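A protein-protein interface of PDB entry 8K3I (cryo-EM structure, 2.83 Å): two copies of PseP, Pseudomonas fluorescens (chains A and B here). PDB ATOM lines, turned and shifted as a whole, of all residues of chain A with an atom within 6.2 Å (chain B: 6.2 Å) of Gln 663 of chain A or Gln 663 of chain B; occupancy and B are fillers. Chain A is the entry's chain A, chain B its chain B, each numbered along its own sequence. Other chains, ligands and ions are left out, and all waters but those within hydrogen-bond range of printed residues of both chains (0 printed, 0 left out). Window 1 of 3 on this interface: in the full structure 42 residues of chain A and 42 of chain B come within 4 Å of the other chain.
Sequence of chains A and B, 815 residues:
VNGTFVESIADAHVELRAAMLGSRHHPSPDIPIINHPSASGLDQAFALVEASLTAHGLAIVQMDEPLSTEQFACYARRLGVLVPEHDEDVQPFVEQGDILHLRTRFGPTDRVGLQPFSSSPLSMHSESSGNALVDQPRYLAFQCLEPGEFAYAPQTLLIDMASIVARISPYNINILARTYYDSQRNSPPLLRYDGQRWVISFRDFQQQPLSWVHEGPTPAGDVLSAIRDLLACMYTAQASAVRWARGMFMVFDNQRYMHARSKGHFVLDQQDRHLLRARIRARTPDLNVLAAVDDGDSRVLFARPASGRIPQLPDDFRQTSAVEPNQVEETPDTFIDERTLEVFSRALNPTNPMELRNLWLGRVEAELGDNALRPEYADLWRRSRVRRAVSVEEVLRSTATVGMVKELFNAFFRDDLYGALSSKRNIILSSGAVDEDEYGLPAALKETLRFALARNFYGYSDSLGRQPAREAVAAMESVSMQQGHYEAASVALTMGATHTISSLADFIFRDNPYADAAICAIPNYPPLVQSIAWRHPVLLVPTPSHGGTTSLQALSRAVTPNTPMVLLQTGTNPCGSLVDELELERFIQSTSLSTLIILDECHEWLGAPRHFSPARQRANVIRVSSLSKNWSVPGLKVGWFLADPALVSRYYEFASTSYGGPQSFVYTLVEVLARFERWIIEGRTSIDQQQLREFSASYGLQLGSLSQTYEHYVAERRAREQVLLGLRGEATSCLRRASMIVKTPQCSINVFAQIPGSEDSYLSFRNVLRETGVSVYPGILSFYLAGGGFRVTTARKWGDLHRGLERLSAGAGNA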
ATOM      1  N   SER A 461     -18.055  12.484   7.093  1.00  0.00           N
ATOM      2  CA  SER A 461     -18.371  13.892   6.920  1.00  0.00           C
ATOM      3  C   SER A 461     -18.430  14.238   5.439  1.00  0.00           C
ATOM      4  O   SER A 461     -17.956  13.491   4.580  1.00  0.00           O
ATOM      5  CB  SER A 461     -17.338  14.775   7.620  1.00  0.00           C
ATOM      6  OG  SER A 461     -16.087  14.717   6.959  1.00  0.00           O
ATOM      7  N   THR A 494     -10.226  21.787   4.408  1.00  0.00           N
ATOM      8  CA  THR A 494      -9.218  20.920   3.816  1.00  0.00           C
ATOM      9  C   THR A 494      -8.243  20.469   4.901  1.00  0.00           C
ATOM     10  O   THR A 494      -8.331  20.884   6.061  1.00  0.00           O
ATOM     11  CB  THR A 494      -8.471  21.633   2.683  1.00  0.00           C
ATOM     12  OG1 THR A 494      -7.789  22.777   3.206  1.00  0.00           O
ATOM     13  CG2 THR A 494      -9.431  22.087   1.594  1.00  0.00           C
ATOM     14  N   MET A 495      -7.313  19.597   4.518  1.00  0.00           N
ATOM     15  CA  MET A 495      -6.316  19.053   5.443  1.00  0.00           C
ATOM     16  C   MET A 495      -4.958  19.729   5.243  1.00  0.00           C
ATOM     17  O   MET A 495      -3.968  19.106   4.868  1.00  0.00           O
ATOM     18  CB  MET A 495      -6.215  17.541   5.273  1.00  0.00           C
ATOM     19  CG  MET A 495      -7.494  16.795   5.630  1.00  0.00           C
ATOM     20  SD  MET A 495      -7.386  15.023   5.352  1.00  0.00           S
ATOM     21  CE  MET A 495      -6.966  14.985   3.615  1.00  0.00           C
ATOM     22  N   PRO A 634       0.617  21.734  13.174  1.00  0.00           N
ATOM     23  CA  PRO A 634       0.823  21.061  11.882  1.00  0.00           C
ATOM     24  C   PRO A 634       0.365  19.614  11.880  1.00  0.00           C
ATOM     25  O   PRO A 634      -0.015  19.095  10.826  1.00  0.00           O
ATOM     26  CB  PRO A 634       2.341  21.164  11.675  1.00  0.00           C
ATOM     27  CG  PRO A 634       2.799  22.194  12.640  1.00  0.00           C
ATOM     28  CD  PRO A 634       1.899  22.062  13.809  1.00  0.00           C
ATOM     29  N   GLY A 635       0.403  18.946  13.035  1.00  0.00           N
ATOM     30  CA  GLY A 635       0.054  17.540  13.090  1.00  0.00           C
ATOM     31  C   GLY A 635      -1.435  17.272  13.038  1.00  0.00           C
ATOM     32  O   GLY A 635      -1.850  16.140  12.784  1.00  0.00           O
ATOM     33  N   LEU A 636      -2.258  18.292  13.292  1.00  0.00           N
ATOM     34  CA  LEU A 636      -3.699  18.120  13.134  1.00  0.00           C
ATOM     35  C   LEU A 636      -4.114  18.155  11.671  1.00  0.00           C
ATOM     36  O   LEU A 636      -5.088  17.495  11.294  1.00  0.00           O
ATOM     37  CB  LEU A 636      -4.459  19.185  13.923  1.00  0.00           C
ATOM     38  CG  LEU A 636      -4.569  18.951  15.430  1.00  0.00           C
ATOM     39  CD1 LEU A 636      -5.344  20.072  16.092  1.00  0.00           C
ATOM     40  CD2 LEU A 636      -5.221  17.613  15.719  1.00  0.00           C
ATOM     41  N   LYS A 637      -3.399  18.914  10.842  1.00  0.00           N
ATOM     42  CA  LYS A 637      -3.688  19.045   9.412  1.00  0.00           C
ATOM     43  C   LYS A 637      -5.102  19.578   9.175  1.00  0.00           C
ATOM     44  O   LYS A 637      -5.967  18.902   8.620  1.00  0.00           O
ATOM     45  CB  LYS A 637      -3.470  17.715   8.684  1.00  0.00           C
ATOM     46  CG  LYS A 637      -2.059  17.177   8.803  1.00  0.00           C
ATOM     47  CD  LYS A 637      -1.876  15.926   7.981  1.00  0.00           C
ATOM     48  CE  LYS A 637      -1.725  16.256   6.514  1.00  0.00           C
ATOM     49  NZ  LYS A 637      -0.441  16.944   6.237  1.00  0.00           N
ATOM     50  N   VAL A 638      -5.322  20.815   9.609  1.00  0.00           N
ATOM     51  CA  VAL A 638      -6.596  21.505   9.446  1.00  0.00           C
ATOM     52  C   VAL A 638      -6.355  22.798   8.684  1.00  0.00           C
ATOM     53  O   VAL A 638      -5.453  23.567   9.028  1.00  0.00           O
ATOM     54  CB  VAL A 638      -7.264  21.800  10.800  1.00  0.00           C
ATOM     55  CG1 VAL A 638      -8.607  22.467  10.589  1.00  0.00           C
ATOM     56  CG2 VAL A 638      -7.422  20.532  11.598  1.00  0.00           C
ATOM     57  N   GLY A 661     -13.390  13.908   1.752  1.00  0.00           N
ATOM     58  CA  GLY A 661     -13.656  14.954   2.709  1.00  0.00           C
ATOM     59  C   GLY A 661     -12.643  15.029   3.833  1.00  0.00           C
ATOM     60  O   GLY A 661     -11.816  14.133   4.018  1.00  0.00           O
ATOM     61  N   PRO A 662     -12.692  16.106   4.605  1.00  0.00           N
ATOM     62  CA  PRO A 662     -11.737  16.304   5.697  1.00  0.00           C
ATOM     63  C   PRO A 662     -12.169  15.551   6.952  1.00  0.00           C
ATOM     64  O   PRO A 662     -13.203  14.891   6.989  1.00  0.00           O
ATOM     65  CB  PRO A 662     -11.777  17.815   5.905  1.00  0.00           C
ATOM     66  CG  PRO A 662     -13.177  18.170   5.566  1.00  0.00           C
ATOM     67  CD  PRO A 662     -13.543  17.291   4.406  1.00  0.00           C
ATOM     68  N   GLN A 663     -11.353  15.672   7.994  1.00  0.00           N
ATOM     69  CA  GLN A 663     -11.654  15.020   9.261  1.00  0.00           C
ATOM     70  C   GLN A 663     -12.863  15.681   9.906  1.00  0.00           C
ATOM     71  O   GLN A 663     -12.880  16.899  10.106  1.00  0.00           O
ATOM     72  CB  GLN A 663     -10.455  15.094  10.204  1.00  0.00           C
ATOM     73  CG  GLN A 663      -9.129  14.702   9.596  1.00  0.00           C
ATOM     74  CD  GLN A 663      -8.169  15.869   9.513  1.00  0.00           C
ATOM     75  OE1 GLN A 663      -8.571  17.004   9.262  1.00  0.00           O
ATOM     76  NE2 GLN A 663      -6.890  15.598   9.735  1.00  0.00           N
ATOM     77  N   SER A 664     -13.878  14.882  10.230  1.00  0.00           N
ATOM     78  CA  SER A 664     -14.994  15.408  11.002  1.00  0.00           C
ATOM     79  C   SER A 664     -14.578  15.684  12.436  1.00  0.00           C
ATOM     80  O   SER A 664     -15.132  16.577  13.088  1.00  0.00           O
ATOM     81  CB  SER A 664     -16.166  14.431  10.967  1.00  0.00           C
ATOM     82  OG  SER A 664     -15.854  13.237  11.659  1.00  0.00           O
ATOM     83  N   PHE A 665     -13.567  14.961  12.916  1.00  0.00           N
ATOM     84  CA  PHE A 665     -13.161  15.011  14.313  1.00  0.00           C
ATOM     85  C   PHE A 665     -12.716  16.403  14.743  1.00  0.00           C
ATOM     86  O   PHE A 665     -12.698  16.692  15.943  1.00  0.00           O
ATOM     87  CB  PHE A 665     -12.052  13.977  14.529  1.00  0.00           C
ATOM     88  CG  PHE A 665     -11.412  14.030  15.879  1.00  0.00           C
ATOM     89  CD1 PHE A 665     -12.056  13.509  16.983  1.00  0.00           C
ATOM     90  CD2 PHE A 665     -10.149  14.565  16.037  1.00  0.00           C
ATOM     91  CE1 PHE A 665     -11.465  13.544  18.225  1.00  0.00           C
ATOM     92  CE2 PHE A 665      -9.551  14.602  17.271  1.00  0.00           C
ATOM     93  CZ  PHE A 665     -10.209  14.090  18.371  1.00  0.00           C
ATOM     94  N   VAL A 666     -12.379  17.282  13.797  1.00  0.00           N
ATOM     95  CA  VAL A 666     -11.902  18.619  14.126  1.00  0.00           C
ATOM     96  C   VAL A 666     -12.961  19.693  13.921  1.00  0.00           C
ATOM     97  O   VAL A 666     -12.714  20.856  14.271  1.00  0.00           O
ATOM     98  CB  VAL A 666     -10.635  18.970  13.320  1.00  0.00           C
ATOM     99  CG1 VAL A 666      -9.514  18.012  13.653  1.00  0.00           C
ATOM    100  CG2 VAL A 666     -10.929  18.964  11.831  1.00  0.00           C
ATOM    101  N   TYR A 667     -14.140  19.340  13.393  1.00  0.00           N
ATOM    102  CA  TYR A 667     -15.133  20.350  13.030  1.00  0.00           C
ATOM    103  C   TYR A 667     -15.443  21.280  14.193  1.00  0.00           C
ATOM    104  O   TYR A 667     -15.376  22.507  14.056  1.00  0.00           O
ATOM    105  CB  TYR A 667     -16.420  19.681  12.546  1.00  0.00           C
ATOM    106  CG  TYR A 667     -16.342  19.139  11.148  1.00  0.00           C
ATOM    107  CD1 TYR A 667     -15.340  19.545  10.284  1.00  0.00           C
ATOM    108  CD2 TYR A 667     -17.263  18.209  10.695  1.00  0.00           C
ATOM    109  CE1 TYR A 667     -15.263  19.045   9.003  1.00  0.00           C
ATOM    110  CE2 TYR A 667     -17.192  17.705   9.417  1.00  0.00           C
ATOM    111  CZ  TYR A 667     -16.189  18.125   8.576  1.00  0.00           C
ATOM    112  OH  TYR A 667     -16.108  17.625   7.304  1.00  0.00           O
ATOM    113  N   SER B 461       5.643  15.753  11.256  1.00  0.00           N
ATOM    114  CA  SER B 461       6.021  14.351  11.222  1.00  0.00           C
ATOM    115  C   SER B 461       6.567  13.990   9.848  1.00  0.00           C
ATOM    116  O   SER B 461       6.413  14.732   8.875  1.00  0.00           O
ATOM    117  CB  SER B 461       4.830  13.454  11.561  1.00  0.00           C
ATOM    118  OG  SER B 461       3.869  13.471  10.520  1.00  0.00           O
ATOM    119  N   THR B 494      -0.835   6.428   6.141  1.00  0.00           N
ATOM    120  CA  THR B 494      -1.582   7.285   5.232  1.00  0.00           C
ATOM    121  C   THR B 494      -2.865   7.748   5.917  1.00  0.00           C
ATOM    122  O   THR B 494      -3.173   7.352   7.045  1.00  0.00           O
ATOM    123  CB  THR B 494      -1.902   6.555   3.923  1.00  0.00           C
ATOM    124  OG1 THR B 494      -2.725   5.418   4.200  1.00  0.00           O
ATOM    125  CG2 THR B 494      -0.632   6.087   3.230  1.00  0.00           C
ATOM    126  N   MET B 495      -3.609   8.611   5.227  1.00  0.00           N
ATOM    127  CA  MET B 495      -4.856   9.170   5.753  1.00  0.00           C
ATOM    128  C   MET B 495      -6.070   8.485   5.124  1.00  0.00           C
ATOM    129  O   MET B 495      -6.870   9.095   4.419  1.00  0.00           O
ATOM    130  CB  MET B 495      -4.889  10.678   5.528  1.00  0.00           C
ATOM    131  CG  MET B 495      -3.791  11.432   6.263  1.00  0.00           C
ATOM    132  SD  MET B 495      -3.832  13.203   5.962  1.00  0.00           S
ATOM    133  CE  MET B 495      -3.622  13.241   4.189  1.00  0.00           C
ATOM    134  N   PRO B 634     -14.012   6.550  10.682  1.00  0.00           N
ATOM    135  CA  PRO B 634     -13.763   7.208   9.390  1.00  0.00           C
ATOM    136  C   PRO B 634     -13.331   8.655   9.529  1.00  0.00           C
ATOM    137  O   PRO B 634     -12.613   9.165   8.662  1.00  0.00           O
ATOM    138  CB  PRO B 634     -15.119   7.097   8.676  1.00  0.00           C
ATOM    139  CG  PRO B 634     -15.881   6.080   9.439  1.00  0.00           C
ATOM    140  CD  PRO B 634     -15.434   6.225  10.844  1.00  0.00           C
ATOM    141  N   GLY B 635     -13.759   9.335  10.593  1.00  0.00           N
ATOM    142  CA  GLY B 635     -13.447  10.743  10.749  1.00  0.00           C
ATOM    143  C   GLY B 635     -12.029  11.014  11.206  1.00  0.00           C
ATOM    144  O   GLY B 635     -11.551  12.144  11.099  1.00  0.00           O
ATOM    145  N   LEU B 636     -11.344   9.998  11.736  1.00  0.00           N
ATOM    146  CA  LEU B 636      -9.936  10.171  12.078  1.00  0.00           C
ATOM    147  C   LEU B 636      -9.046  10.121  10.844  1.00  0.00           C
ATOM    148  O   LEU B 636      -8.002  10.779  10.815  1.00  0.00           O
ATOM    149  CB  LEU B 636      -9.493   9.115  13.090  1.00  0.00           C
ATOM    150  CG  LEU B 636      -9.904   9.364  14.541  1.00  0.00           C
ATOM    151  CD1 LEU B 636      -9.403   8.252  15.439  1.00  0.00           C
ATOM    152  CD2 LEU B 636      -9.389  10.707  15.022  1.00  0.00           C
ATOM    153  N   LYS B 637      -9.437   9.352   9.829  1.00  0.00           N
ATOM    154  CA  LYS B 637      -8.678   9.207   8.585  1.00  0.00           C
ATOM    155  C   LYS B 637      -7.268   8.674   8.850  1.00  0.00           C
ATOM    156  O   LYS B 637      -6.264   9.346   8.619  1.00  0.00           O
ATOM    157  CB  LYS B 637      -8.632  10.530   7.813  1.00  0.00           C
ATOM    158  CG  LYS B 637      -9.998  11.066   7.439  1.00  0.00           C
ATOM    159  CD  LYS B 637      -9.888  12.308   6.591  1.00  0.00           C
ATOM    160  CE  LYS B 637      -9.527  11.964   5.163  1.00  0.00           C
ATOM    161  NZ  LYS B 637     -10.639  11.270   4.472  1.00  0.00           N
ATOM    162  N   VAL B 638      -7.212   7.442   9.347  1.00  0.00           N
ATOM    163  CA  VAL B 638      -5.960   6.753   9.634  1.00  0.00           C
ATOM    164  C   VAL B 638      -5.929   5.453   8.847  1.00  0.00           C
ATOM    165  O   VAL B 638      -6.893   4.682   8.876  1.00  0.00           O
ATOM    166  CB  VAL B 638      -5.793   6.473  11.137  1.00  0.00           C
ATOM    167  CG1 VAL B 638      -4.460   5.805  11.401  1.00  0.00           C
ATOM    168  CG2 VAL B 638      -5.914   7.747  11.928  1.00  0.00           C
ATOM    169  N   GLY B 661       3.067  14.287   4.648  1.00  0.00           N
ATOM    170  CA  GLY B 661       2.987  13.251   5.647  1.00  0.00           C
ATOM    171  C   GLY B 661       1.651  13.186   6.358  1.00  0.00           C
ATOM    172  O   GLY B 661       0.813  14.081   6.241  1.00  0.00           O
ATOM    173  N   PRO B 662       1.432  12.116   7.110  1.00  0.00           N
ATOM    174  CA  PRO B 662       0.161  11.927   7.812  1.00  0.00           C
ATOM    175  C   PRO B 662       0.141  12.691   9.133  1.00  0.00           C
ATOM    176  O   PRO B 662       1.100  13.354   9.514  1.00  0.00           O
ATOM    177  CB  PRO B 662       0.125  10.418   8.037  1.00  0.00           C
ATOM    178  CG  PRO B 662       1.555  10.062   8.199  1.00  0.00           C
ATOM    179  CD  PRO B 662       2.299  10.931   7.227  1.00  0.00           C
ATOM    180  N   GLN B 663      -0.983  12.580   9.834  1.00  0.00           N
ATOM    181  CA  GLN B 663      -1.134  13.245  11.121  1.00  0.00           C
ATOM    182  C   GLN B 663      -0.218  12.593  12.147  1.00  0.00           C
ATOM    183  O   GLN B 663      -0.272  11.376  12.353  1.00  0.00           O
ATOM    184  CB  GLN B 663      -2.581  13.179  11.599  1.00  0.00           C
ATOM    185  CG  GLN B 663      -3.619  13.563  10.570  1.00  0.00           C
ATOM    186  CD  GLN B 663      -4.496  12.394  10.176  1.00  0.00           C
ATOM    187  OE1 GLN B 663      -4.034  11.257  10.089  1.00  0.00           O
ATOM    188  NE2 GLN B 663      -5.773  12.663   9.946  1.00  0.00           N
ATOM    189  N   SER B 664       0.628  13.396  12.789  1.00  0.00           N
ATOM    190  CA  SER B 664       1.413  12.879  13.901  1.00  0.00           C
ATOM    191  C   SER B 664       0.532  12.617  15.110  1.00  0.00           C
ATOM    192  O   SER B 664       0.828  11.731  15.919  1.00  0.00           O
ATOM    193  CB  SER B 664       2.529  13.858  14.257  1.00  0.00           C
ATOM    194  OG  SER B 664       2.001  15.057  14.794  1.00  0.00           O
ATOM    195  N   PHE B 665      -0.581  13.344  15.209  1.00  0.00           N
ATOM    196  CA  PHE B 665      -1.439  13.307  16.384  1.00  0.00           C
ATOM    197  C   PHE B 665      -2.007  11.918  16.651  1.00  0.00           C
ATOM    198  O   PHE B 665      -2.432  11.642  17.777  1.00  0.00           O
ATOM    199  CB  PHE B 665      -2.555  14.340  16.197  1.00  0.00           C
ATOM    200  CG  PHE B 665      -3.617  14.299  17.248  1.00  0.00           C
ATOM    201  CD1 PHE B 665      -3.388  14.834  18.501  1.00  0.00           C
ATOM    202  CD2 PHE B 665      -4.859  13.761  16.972  1.00  0.00           C
ATOM    203  CE1 PHE B 665      -4.368  14.809  19.467  1.00  0.00           C
ATOM    204  CE2 PHE B 665      -5.841  13.734  17.929  1.00  0.00           C
ATOM    205  CZ  PHE B 665      -5.598  14.260  19.180  1.00  0.00           C
ATOM    206  N   VAL B 666      -2.002  11.029  15.656  1.00  0.00           N
ATOM    207  CA  VAL B 666      -2.566   9.695  15.817  1.00  0.00           C
ATOM    208  C   VAL B 666      -1.503   8.620  15.997  1.00  0.00           C
ATOM    209  O   VAL B 666      -1.859   7.462  16.253  1.00  0.00           O
ATOM    210  CB  VAL B 666      -3.482   9.333  14.630  1.00  0.00           C
ATOM    211  CG1 VAL B 666      -4.649  10.293  14.551  1.00  0.00           C
ATOM    212  CG2 VAL B 666      -2.698   9.326  13.332  1.00  0.00           C
ATOM    213  N   TYR B 667      -0.216   8.969  15.901  1.00  0.00           N
ATOM    214  CA  TYR B 667       0.841   7.957  15.908  1.00  0.00           C
ATOM    215  C   TYR B 667       0.733   7.040  17.116  1.00  0.00           C
ATOM    216  O   TYR B 667       0.715   5.810  16.978  1.00  0.00           O
ATOM    217  CB  TYR B 667       2.217   8.621  15.886  1.00  0.00           C
ATOM    218  CG  TYR B 667       2.621   9.149  14.541  1.00  0.00           C
ATOM    219  CD1 TYR B 667       1.970   8.737  13.391  1.00  0.00           C
ATOM    220  CD2 TYR B 667       3.644  10.073  14.420  1.00  0.00           C
ATOM    221  CE1 TYR B 667       2.334   9.224  12.156  1.00  0.00           C
ATOM    222  CE2 TYR B 667       4.015  10.564  13.190  1.00  0.00           C
ATOM    223  CZ  TYR B 667       3.354  10.138  12.062  1.00  0.00           C
ATOM    224  OH  TYR B 667       3.714  10.628  10.834  1.00  0.00           O
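NZ of Lys 637 of chain A sits at hydrogen-bond distance from O of Gly 661 of chain B, 3.1 Å away. The side-chain amino group of Lys 637 of chain B is in hydrogen-bond range of the backbone carbonyl oxygen of Gly 661 of chain A, 3.1 Å away. The side-chain amide nitrogen (NE2) of Gln 663 of chain B lies close to the side-chain amide nitrogen (NE2) of Gln 663 of chain A, 3.1 Å away.
The side-chain hydroxyl (OG) of Ser 461 of chain A lies within hydrogen-bond range of the backbone carbonyl oxygen (O) of Pro 662 of chain A (2.9 Å). NE2 of Gln 663 of chain A lies within hydrogen-bond range of O of Leu 636 of chain A (3.0 Å). The backbone carbonyl oxygen (O) of Lys 637 of chain A lies close to the side-chain amide oxygen (OE1) of Gln 663 of chain A (3.3 Å). The backbone carbonyl oxygen (O) of Pro 662 of chain B is in hydrogen-bond range of the side-chain hydroxyl (OG) of Ser 461 of chain B (2.9 Å). The backbone carbonyl oxygen of Leu 636 of chain B sits at hydrogen-bond distance from the side-chain amide nitrogen of Gln 663 of chain B (3.0 Å). O of Lys 637 of chain B sits close to OE1 of Gln 663 of chain B, 3.3 Å away.
Among the printed residues, merely in contact across the chains: Met 495 of chain A with Met 495 of chain B (3.8 Å), Met 495 of chain A with Lys 637 of chain B (3.7 Å), Gly 635 of chain A with Gln 663 of chain B (3.3 Å), Gly 635 of chain A with Ser 664 of chain B (3.6 Å), Gly 635 of chain A with Phe 665 of chain B (3.9 Å), Leu 636 of chain A with Phe 665 of chain B (3.99 Å), Lys 637 of chain A with Met 495 of chain B (3.8 Å), Lys 637 of chain A with Pro 662 of chain B (3.98 Å), Lys 637 of chain A with Gln 663 of chain B (3.9 Å), Pro 662 of chain A with Lys 637 of chain B (3.98 Å), Gln 663 of chain A with Gly 635 of chain B (3.3 Å), Gln 663 of chain A with Lys 637 of chain B (3.9 Å), Ser 664 of chain A with Gly 635 of chain B (3.6 Å), Phe 665 of chain A with Gly 635 of chain B (3.9 Å), Phe 665 of chain A with Leu 636 of chain B (3.98 Å) and Phe 665 of chain A with Phe 665 of chain B (3.9 Å).
Gln 663 of chain A touches just these residues of chain B: Gly 635, Lys 637 and Gln 663. Of chain A, only Gly 635, Lys 637 and Gln 663 come within 4 Å of Gln 663 of chain B. Printed residues of chain B within 4 Å of Gly 661 of chain A: Lys 637. Of the printed residues of chain A, Phe 665 of chain B touches Gly 635, Leu 636 and Phe 665. Of the printed residues of chain B, Lys 637 of chain A touches Met 495, Gly 661, Pro 662 and Gln 663. Of the printed residues of chain A, Ser 664 of chain B touches Gly 635. Printed residues of chain B within 4 Å of Ser 664 of chain A: Gly 635 (3.6 Å). Val 666 of chain A touches none of the printed residues of chain B. The nearest residue of chain B that does not touch Gln 663 of chain A is Leu 636 of chain B (4.3 Å). The nearest printed residue of chain A that does not touch Leu 636 of chain B is Gln 663 of chain A (4.3 Å).
Of the 15 printed residues of chain A, 9 touch a printed residue of chain B. Printed residues of chain A that touch a printed residue of chain B: Met 495, Gly 635, Leu 636, Lys 637, Gly 661, Pro 662, Gln 663, Ser 664 and Phe 665. Hydrophobic or aromatic side chains of chain A within 4 Å of the printed part of chain B: Met 495, Leu 636 and Phe 665. Among the printed residues, no Asp or Glu carboxylate lies within 4 Å of a Lys or Arg side-chain nitrogen of the other chain.
Met 495 of chain A touches Lys 637 of chain B, and with the chains exchanged Lys 637 of chain A touches Met 495 of chain B. Lys 637 of chain A touches Pro 662 of chain B, and with the chains exchanged Pro 662 of chain A touches Lys 637 of chain B. Lys 637 of chain A touches Gln 663 of chain B, and with the chains exchanged Gln 663 of chain A touches Lys 637 of chain B. Phe 665 of chain B touches its own counterpart, Phe 665 of chain A. Of the 19 pairs that touch across the chains among the printed residues, 19 have their exchanged pair printed and touching as well.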
